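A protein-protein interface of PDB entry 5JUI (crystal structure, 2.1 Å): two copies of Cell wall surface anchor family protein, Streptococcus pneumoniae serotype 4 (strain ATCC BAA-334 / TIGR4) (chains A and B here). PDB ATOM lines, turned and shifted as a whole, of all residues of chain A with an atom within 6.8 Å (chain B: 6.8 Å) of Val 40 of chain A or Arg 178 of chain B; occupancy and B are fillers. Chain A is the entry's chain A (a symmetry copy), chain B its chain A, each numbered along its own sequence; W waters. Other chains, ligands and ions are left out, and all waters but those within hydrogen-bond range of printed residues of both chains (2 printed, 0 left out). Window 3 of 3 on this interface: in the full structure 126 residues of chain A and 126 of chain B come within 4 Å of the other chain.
The backbone carbonyl oxygen (O) of Ala 177 of chain B is in hydrogen-bond range of the backbone NH (N) of Tyr 87 of chain A (2.7 Å).
The backbone carbonyl oxygen (O) of Ser 85 of chain A lies within hydrogen-bond range of the backbone NH (N) of Thr 179 of chain B (3.0 Å).
N of Val 37 of chain A is in hydrogen-bond range of O of Tyr 186 of chain B.
OH of Tyr 84 of chain A sits at hydrogen-bond distance from OH of Tyr 186 of chain B, 2.7 Å away.
O of Ala 176 of chain B lies within hydrogen-bond range of N of Tyr 186 of chain B (2.7 Å).
NH1 of Arg 178 of chain B lies within salt-bridge range of OD1 of Asp 180 of chain B.
The side-chain carboxylate (OD1) of Asp 38 of chain A is in hydrogen-bond range of the backbone NH (N) of Val 40 of chain A (3.0 Å).
OD1 of Asp 38 of chain A lies within hydrogen-bond range of N of Tyr 41 of chain A (3.1 Å).
O of Val 43 of chain A is in hydrogen-bond range of N of Asp 38 of chain A.
The side-chain hydroxyl of Tyr 84 of chain A is in hydrogen-bond range of the side-chain carboxylate of Asp 38 of chain A, 2.7 Å away.
Among the printed residues, merely in contact across the chains: Asp 38 of chain A with Tyr 186 of chain B (3.4 Å), Ser 39 of chain A with Tyr 186 of chain B (3.6 Å), Val 40 of chain A with Arg 178 of chain B (3.5 Å), Val 40 of chain A with Tyr 186 of chain B (3.6 Å), Tyr 84 of chain A with Arg 178 of chain B (3.9 Å), Ser 85 of chain A with Arg 178 of chain B (3.3 Å), Ile 86 of chain A with Ala 177 of chain B (3.2 Å), Tyr 87 of chain A with Ala 176 of chain B (3.2 Å), Tyr 87 of chain A with Thr 179 of chain B (3.6 Å) and Tyr 87 of chain A with Ile 182 of chain B (3.8 Å).
Of the printed residues of chain B, Tyr 84 of chain A touches Arg 178 (3.9 Å) and Tyr 186 (2.7 Å).
Printed residues of chain A within 4 Å of Ala 176 of chain B: Tyr 87.
Of the printed residues of chain A, Ala 177 of chain B touches Ile 86 and Tyr 87.
Of chain A, only Val 40, Tyr 84 and Ser 85 come within 4 Å of Arg 178 of chain B.
Printed residues of chain A within 4 Å of Thr 179 of chain B: Ser 85 (3.0 Å) and Tyr 87 (3.6 Å).
Of the printed residues of chain A, Ile 182 of chain B touches Tyr 87.
The nearest residue of chain B that does not touch Val 40 of chain A is Asp 180 of chain B (6.6 Å).
Hydrophobic or aromatic side chains of chain A that line the printed part of chain B: Val 40, Tyr 84, Ile 86 and Tyr 87.
Of the 10 printed residues of chain B, 6 touch a printed residue of chain A.
Printed residues of chain B that touch a printed residue of chain A: Ala 176, Ala 177, Arg 178, Thr 179, Ile 182 and Tyr 186.
Hydrophobic or aromatic side chains of chain B within 4 Å of the printed part of chain A: Ala 176, Ile 182 and Tyr 186.
Among the printed residues, no Asp or Glu carboxylate lies within 4 Å of a Lys or Arg side-chain nitrogen of the other chain.
No position is printed for both chains.
Of the 14 pairs that touch across the chains among the printed residues, none has its exchanged pair printed and touching as well.
Water W2 lies within hydrogen-bond range of the side-chain hydroxyl of Tyr 87 of chain A (2.7 Å) and the backbone carbonyl oxygen of Thr 179 of chain B (3.1 Å).
Water W1 bridges N of Ser 85 of chain A and OG1 of Thr 179 of chain B.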
ATOM      1  N   VAL A  37      -4.763  -8.758 -27.802  1.00  0.00           N
ATOM      2  CA  VAL A  37      -5.009  -7.441 -28.373  1.00  0.00           C
ATOM      3  C   VAL A  37      -6.156  -6.754 -27.648  1.00  0.00           C
ATOM      4  O   VAL A  37      -7.215  -7.348 -27.445  1.00  0.00           O
ATOM      5  CB  VAL A  37      -5.352  -7.527 -29.882  1.00  0.00           C
ATOM      6  CG1 VAL A  37      -5.515  -6.138 -30.477  1.00  0.00           C
ATOM      7  CG2 VAL A  37      -4.286  -8.307 -30.630  1.00  0.00           C
ATOM      8  N   ASP A  38      -5.930  -5.512 -27.231  1.00  0.00           N
ATOM      9  CA  ASP A  38      -7.009  -4.685 -26.716  1.00  0.00           C
ATOM     10  C   ASP A  38      -7.786  -4.201 -27.936  1.00  0.00           C
ATOM     11  O   ASP A  38      -7.284  -3.387 -28.711  1.00  0.00           O
ATOM     12  CB  ASP A  38      -6.453  -3.502 -25.914  1.00  0.00           C
ATOM     13  CG  ASP A  38      -7.547  -2.663 -25.262  1.00  0.00           C
ATOM     14  OD1 ASP A  38      -8.497  -2.256 -25.961  1.00  0.00           O
ATOM     15  OD2 ASP A  38      -7.454  -2.387 -24.048  1.00  0.00           O
ATOM     16  N   SER A  39      -8.999  -4.719 -28.107  1.00  0.00           N
ATOM     17  CA  SER A  39      -9.826  -4.432 -29.279  1.00  0.00           C
ATOM     18  C   SER A  39     -10.186  -2.955 -29.389  1.00  0.00           C
ATOM     19  O   SER A  39     -10.269  -2.410 -30.490  1.00  0.00           O
ATOM     20  CB  SER A  39     -11.112  -5.260 -29.236  1.00  0.00           C
ATOM     21  OG  SER A  39     -10.832  -6.636 -29.061  1.00  0.00           O
ATOM     22  N   VAL A  40     -10.404  -2.316 -28.244  1.00  0.00           N
ATOM     23  CA  VAL A  40     -10.838  -0.927 -28.210  1.00  0.00           C
ATOM     24  C   VAL A  40      -9.751   0.022 -28.703  1.00  0.00           C
ATOM     25  O   VAL A  40     -10.011   0.896 -29.527  1.00  0.00           O
ATOM     26  CB  VAL A  40     -11.270  -0.519 -26.791  1.00  0.00           C
ATOM     27  CG1 VAL A  40     -11.578   0.967 -26.732  1.00  0.00           C
ATOM     28  CG2 VAL A  40     -12.480  -1.322 -26.364  1.00  0.00           C
ATOM     29  N   TYR A  41      -8.533  -0.148 -28.203  1.00  0.00           N
ATOM     30  CA  TYR A  41      -7.458   0.764 -28.568  1.00  0.00           C
ATOM     31  C   TYR A  41      -6.475   0.175 -29.577  1.00  0.00           C
ATOM     32  O   TYR A  41      -5.494   0.828 -29.941  1.00  0.00           O
ATOM     33  CB  TYR A  41      -6.732   1.265 -27.317  1.00  0.00           C
ATOM     34  CG  TYR A  41      -7.619   2.138 -26.464  1.00  0.00           C
ATOM     35  CD1 TYR A  41      -7.800   3.479 -26.766  1.00  0.00           C
ATOM     36  CD2 TYR A  41      -8.281   1.621 -25.363  1.00  0.00           C
ATOM     37  CE1 TYR A  41      -8.622   4.280 -25.998  1.00  0.00           C
ATOM     38  CE2 TYR A  41      -9.101   2.415 -24.584  1.00  0.00           C
ATOM     39  CZ  TYR A  41      -9.267   3.743 -24.907  1.00  0.00           C
ATOM     40  OH  TYR A  41     -10.082   4.539 -24.137  1.00  0.00           O
ATOM     41  N   ARG A  42      -6.750  -1.048 -30.025  1.00  0.00           N
ATOM     42  CA  ARG A  42      -5.917  -1.728 -31.019  1.00  0.00           C
ATOM     43  C   ARG A  42      -4.441  -1.715 -30.644  1.00  0.00           C
ATOM     44  O   ARG A  42      -3.590  -1.304 -31.434  1.00  0.00           O
ATOM     45  CB  ARG A  42      -6.115  -1.137 -32.418  1.00  0.00           C
ATOM     46  CG  ARG A  42      -7.564  -0.938 -32.834  1.00  0.00           C
ATOM     47  CD  ARG A  42      -7.741  -1.391 -34.269  1.00  0.00           C
ATOM     48  NE  ARG A  42      -7.029  -0.525 -35.203  1.00  0.00           N
ATOM     49  CZ  ARG A  42      -6.883  -0.783 -36.499  1.00  0.00           C
ATOM     50  NH1 ARG A  42      -7.387  -1.894 -37.017  1.00  0.00           N
ATOM     51  NH2 ARG A  42      -6.218   0.063 -37.272  1.00  0.00           N
ATOM     52  N   VAL A  43      -4.145  -2.152 -29.426  1.00  0.00           N
ATOM     53  CA  VAL A  43      -2.767  -2.250 -28.979  1.00  0.00           C
ATOM     54  C   VAL A  43      -2.566  -3.619 -28.363  1.00  0.00           C
ATOM     55  O   VAL A  43      -3.533  -4.276 -27.973  1.00  0.00           O
ATOM     56  CB  VAL A  43      -2.437  -1.171 -27.926  1.00  0.00           C
ATOM     57  CG1 VAL A  43      -2.317   0.192 -28.586  1.00  0.00           C
ATOM     58  CG2 VAL A  43      -3.499  -1.155 -26.830  1.00  0.00           C
ATOM     59  N   ARG A  81      -8.449   6.644 -22.466  1.00  0.00           N
ATOM     60  CA  ARG A  81      -9.077   7.585 -21.551  1.00  0.00           C
ATOM     61  C   ARG A  81      -8.868   7.084 -20.130  1.00  0.00           C
ATOM     62  O   ARG A  81      -8.775   5.876 -19.898  1.00  0.00           O
ATOM     63  CB  ARG A  81     -10.566   7.768 -21.870  1.00  0.00           C
ATOM     64  CG  ARG A  81     -11.469   6.699 -21.292  1.00  0.00           C
ATOM     65  CD  ARG A  81     -12.931   6.988 -21.584  1.00  0.00           C
ATOM     66  NE  ARG A  81     -13.804   6.005 -20.952  1.00  0.00           N
ATOM     67  CZ  ARG A  81     -14.203   4.877 -21.534  1.00  0.00           C
ATOM     68  NH1 ARG A  81     -13.805   4.586 -22.765  1.00  0.00           N
ATOM     69  NH2 ARG A  81     -14.998   4.040 -20.882  1.00  0.00           N
ATOM     70  N   TYR A  84     -11.338   4.471 -18.725  1.00  0.00           N
ATOM     71  CA  TYR A  84     -11.341   3.136 -19.323  1.00  0.00           C
ATOM     72  C   TYR A  84     -10.849   2.145 -18.281  1.00  0.00           C
ATOM     73  O   TYR A  84      -9.889   2.426 -17.570  1.00  0.00           O
ATOM     74  CB  TYR A  84     -10.417   3.109 -20.542  1.00  0.00           C
ATOM     75  CG  TYR A  84     -10.298   1.770 -21.241  1.00  0.00           C
ATOM     76  CD1 TYR A  84     -11.356   1.240 -21.964  1.00  0.00           C
ATOM     77  CD2 TYR A  84      -9.113   1.048 -21.198  1.00  0.00           C
ATOM     78  CE1 TYR A  84     -11.240   0.023 -22.613  1.00  0.00           C
ATOM     79  CE2 TYR A  84      -8.989  -0.167 -21.846  1.00  0.00           C
ATOM     80  CZ  TYR A  84     -10.055  -0.673 -22.549  1.00  0.00           C
ATOM     81  OH  TYR A  84      -9.935  -1.881 -23.195  1.00  0.00           O
ATOM     82  N   SER A  85     -11.511   0.997 -18.181  1.00  0.00           N
ATOM     83  CA  SER A  85     -11.175   0.005 -17.164  1.00  0.00           C
ATOM     84  C   SER A  85     -11.221  -1.420 -17.705  1.00  0.00           C
ATOM     85  O   SER A  85     -12.053  -1.742 -18.551  1.00  0.00           O
ATOM     86  CB  SER A  85     -12.130   0.126 -15.974  1.00  0.00           C
ATOM     87  OG  SER A  85     -11.677   1.095 -15.048  1.00  0.00           O
ATOM     88  N   ILE A  86     -10.328  -2.270 -17.201  1.00  0.00           N
ATOM     89  CA  ILE A  86     -10.286  -3.673 -17.605  1.00  0.00           C
ATOM     90  C   ILE A  86     -10.307  -4.632 -16.416  1.00  0.00           C
ATOM     91  O   ILE A  86      -9.821  -4.308 -15.334  1.00  0.00           O
ATOM     92  CB  ILE A  86      -9.036  -3.989 -18.466  1.00  0.00           C
ATOM     93  CG1 ILE A  86      -7.756  -3.722 -17.671  1.00  0.00           C
ATOM     94  CG2 ILE A  86      -9.031  -3.161 -19.741  1.00  0.00           C
ATOM     95  CD1 ILE A  86      -6.497  -4.209 -18.359  1.00  0.00           C
ATOM     96  N   TYR A  87     -10.891  -5.809 -16.624  1.00  0.00           N
ATOM     97  CA  TYR A  87     -10.834  -6.885 -15.642  1.00  0.00           C
ATOM     98  C   TYR A  87      -9.675  -7.811 -16.012  1.00  0.00           C
ATOM     99  O   TYR A  87      -9.248  -7.833 -17.168  1.00  0.00           O
ATOM    100  CB  TYR A  87     -12.139  -7.686 -15.643  1.00  0.00           C
ATOM    101  CG  TYR A  87     -13.346  -6.981 -15.053  1.00  0.00           C
ATOM    102  CD1 TYR A  87     -13.287  -6.372 -13.808  1.00  0.00           C
ATOM    103  CD2 TYR A  87     -14.556  -6.955 -15.734  1.00  0.00           C
ATOM    104  CE1 TYR A  87     -14.398  -5.742 -13.263  1.00  0.00           C
ATOM    105  CE2 TYR A  87     -15.672  -6.327 -15.200  1.00  0.00           C
ATOM    106  CZ  TYR A  87     -15.585  -5.722 -13.964  1.00  0.00           C
ATOM    107  OH  TYR A  87     -16.689  -5.097 -13.432  1.00  0.00           O
ATOM    108  N   ALA B 176      -8.534 -10.978 -19.941  1.00  0.00           N
ATOM    109  CA  ALA B 176      -8.602  -9.531 -19.839  1.00  0.00           C
ATOM    110  C   ALA B 176      -9.745  -9.027 -20.705  1.00  0.00           C
ATOM    111  O   ALA B 176      -9.907  -9.458 -21.847  1.00  0.00           O
ATOM    112  CB  ALA B 176      -7.286  -8.897 -20.268  1.00  0.00           C
ATOM    113  N   ALA B 177     -10.539  -8.116 -20.157  1.00  0.00           N
ATOM    114  CA  ALA B 177     -11.690  -7.578 -20.865  1.00  0.00           C
ATOM    115  C   ALA B 177     -12.066  -6.230 -20.278  1.00  0.00           C
ATOM    116  O   ALA B 177     -11.871  -5.996 -19.085  1.00  0.00           O
ATOM    117  CB  ALA B 177     -12.870  -8.539 -20.763  1.00  0.00           C
ATOM    118  N   ARG B 178     -12.608  -5.345 -21.107  1.00  0.00           N
ATOM    119  CA  ARG B 178     -13.121  -4.083 -20.592  1.00  0.00           C
ATOM    120  C   ARG B 178     -14.333  -4.331 -19.698  1.00  0.00           C
ATOM    121  O   ARG B 178     -15.081  -5.291 -19.903  1.00  0.00           O
ATOM    122  CB  ARG B 178     -13.443  -3.103 -21.722  1.00  0.00           C
ATOM    123  CG  ARG B 178     -14.427  -3.604 -22.766  1.00  0.00           C
ATOM    124  CD  ARG B 178     -14.611  -2.539 -23.835  1.00  0.00           C
ATOM    125  NE  ARG B 178     -15.341  -3.018 -25.005  1.00  0.00           N
ATOM    126  CZ  ARG B 178     -16.466  -2.473 -25.455  1.00  0.00           C
ATOM    127  NH1 ARG B 178     -16.991  -1.424 -24.836  1.00  0.00           N
ATOM    128  NH2 ARG B 178     -17.064  -2.971 -26.529  1.00  0.00           N
ATOM    129  N   THR B 179     -14.504  -3.477 -18.696  1.00  0.00           N
ATOM    130  CA  THR B 179     -15.487  -3.708 -17.641  1.00  0.00           C
ATOM    131  C   THR B 179     -16.949  -3.664 -18.095  1.00  0.00           C
ATOM    132  O   THR B 179     -17.818  -4.197 -17.406  1.00  0.00           O
ATOM    133  CB  THR B 179     -15.286  -2.730 -16.468  1.00  0.00           C
ATOM    134  OG1 THR B 179     -15.231  -1.387 -16.964  1.00  0.00           O
ATOM    135  CG2 THR B 179     -13.981  -3.046 -15.737  1.00  0.00           C
ATOM    136  N   ASP B 180     -17.224  -3.041 -19.240  1.00  0.00           N
ATOM    137  CA  ASP B 180     -18.600  -2.970 -19.738  1.00  0.00           C
ATOM    138  C   ASP B 180     -18.865  -4.003 -20.834  1.00  0.00           C
ATOM    139  O   ASP B 180     -19.916  -3.992 -21.474  1.00  0.00           O
ATOM    140  CB  ASP B 180     -18.933  -1.563 -20.244  1.00  0.00           C
ATOM    141  CG  ASP B 180     -18.018  -1.115 -21.372  1.00  0.00           C
ATOM    142  OD1 ASP B 180     -16.975  -1.763 -21.596  1.00  0.00           O
ATOM    143  OD2 ASP B 180     -18.344  -0.112 -22.040  1.00  0.00           O
ATOM    144  N   ARG B 181     -17.908  -4.905 -21.024  1.00  0.00           N
ATOM    145  CA  ARG B 181     -18.036  -5.998 -21.980  1.00  0.00           C
ATOM    146  C   ARG B 181     -17.124  -7.138 -21.543  1.00  0.00           C
ATOM    147  O   ARG B 181     -16.109  -7.423 -22.182  1.00  0.00           O
ATOM    148  CB  ARG B 181     -17.690  -5.523 -23.395  1.00  0.00           C
ATOM    149  CG  ARG B 181     -18.050  -6.508 -24.502  1.00  0.00           C
ATOM    150  CD  ARG B 181     -19.544  -6.775 -24.593  1.00  0.00           C
ATOM    151  NE  ARG B 181     -19.871  -7.644 -25.723  1.00  0.00           N
ATOM    152  CZ  ARG B 181     -20.121  -8.946 -25.619  1.00  0.00           C
ATOM    153  NH1 ARG B 181     -20.077  -9.538 -24.434  1.00  0.00           N
ATOM    154  NH2 ARG B 181     -20.409  -9.659 -26.701  1.00  0.00           N
ATOM    155  N   ILE B 182     -17.496  -7.780 -20.439  1.00  0.00           N
ATOM    156  CA  ILE B 182     -16.660  -8.783 -19.791  1.00  0.00           C
ATOM    157  C   ILE B 182     -16.498 -10.031 -20.659  1.00  0.00           C
ATOM    158  O   ILE B 182     -15.542 -10.789 -20.494  1.00  0.00           O
ATOM    159  CB  ILE B 182     -17.207  -9.160 -18.387  1.00  0.00           C
ATOM    160  CG1 ILE B 182     -16.135  -9.878 -17.560  1.00  0.00           C
ATOM    161  CG2 ILE B 182     -18.478  -9.998 -18.500  1.00  0.00           C
ATOM    162  CD1 ILE B 182     -16.564 -10.208 -16.139  1.00  0.00           C
ATOM    163  N   GLY B 183     -17.425 -10.228 -21.591  1.00  0.00           N
ATOM    164  CA  GLY B 183     -17.468 -11.441 -22.388  1.00  0.00           C
ATOM    165  C   GLY B 183     -16.386 -11.575 -23.445  1.00  0.00           C
ATOM    166  O   GLY B 183     -16.087 -12.684 -23.887  1.00  0.00           O
ATOM    167  N   ILE B 184     -15.799 -10.455 -23.854  1.00  0.00           N
ATOM    168  CA  ILE B 184     -14.788 -10.474 -24.909  1.00  0.00           C
ATOM    169  C   ILE B 184     -13.376 -10.525 -24.321  1.00  0.00           C
ATOM    170  O   ILE B 184     -12.853  -9.514 -23.848  1.00  0.00           O
ATOM    171  CB  ILE B 184     -14.911  -9.248 -25.829  1.00  0.00           C
ATOM    172  CG1 ILE B 184     -16.356  -9.079 -26.308  1.00  0.00           C
ATOM    173  CG2 ILE B 184     -13.964  -9.374 -27.014  1.00  0.00           C
ATOM    174  CD1 ILE B 184     -16.896 -10.265 -27.079  1.00  0.00           C
ATOM    175  N   TYR B 186      -9.561 -10.438 -24.374  1.00  0.00           N
ATOM    176  CA  TYR B 186      -8.485  -9.874 -25.187  1.00  0.00           C
ATOM    177  C   TYR B 186      -7.385 -10.878 -25.539  1.00  0.00           C
ATOM    178  O   TYR B 186      -6.631 -10.668 -26.488  1.00  0.00           O
ATOM    179  CB  TYR B 186      -7.867  -8.662 -24.481  1.00  0.00           C
ATOM    180  CG  TYR B 186      -8.739  -7.420 -24.454  1.00  0.00           C
ATOM    181  CD1 TYR B 186      -9.845  -7.290 -25.286  1.00  0.00           C
ATOM    182  CD2 TYR B 186      -8.445  -6.371 -23.595  1.00  0.00           C
ATOM    183  CE1 TYR B 186     -10.634  -6.147 -25.256  1.00  0.00           C
ATOM    184  CE2 TYR B 186      -9.225  -5.230 -23.560  1.00  0.00           C
ATOM    185  CZ  TYR B 186     -10.317  -5.124 -24.393  1.00  0.00           C
ATOM    186  OH  TYR B 186     -11.093  -3.986 -24.354  1.00  0.00           O
HETATM  187  O   HOH W   1     -14.385   0.579 -19.252  1.00  0.00           O
HETATM  188  O   HOH W   2     -19.066  -4.991 -14.645  1.00  0.00           O
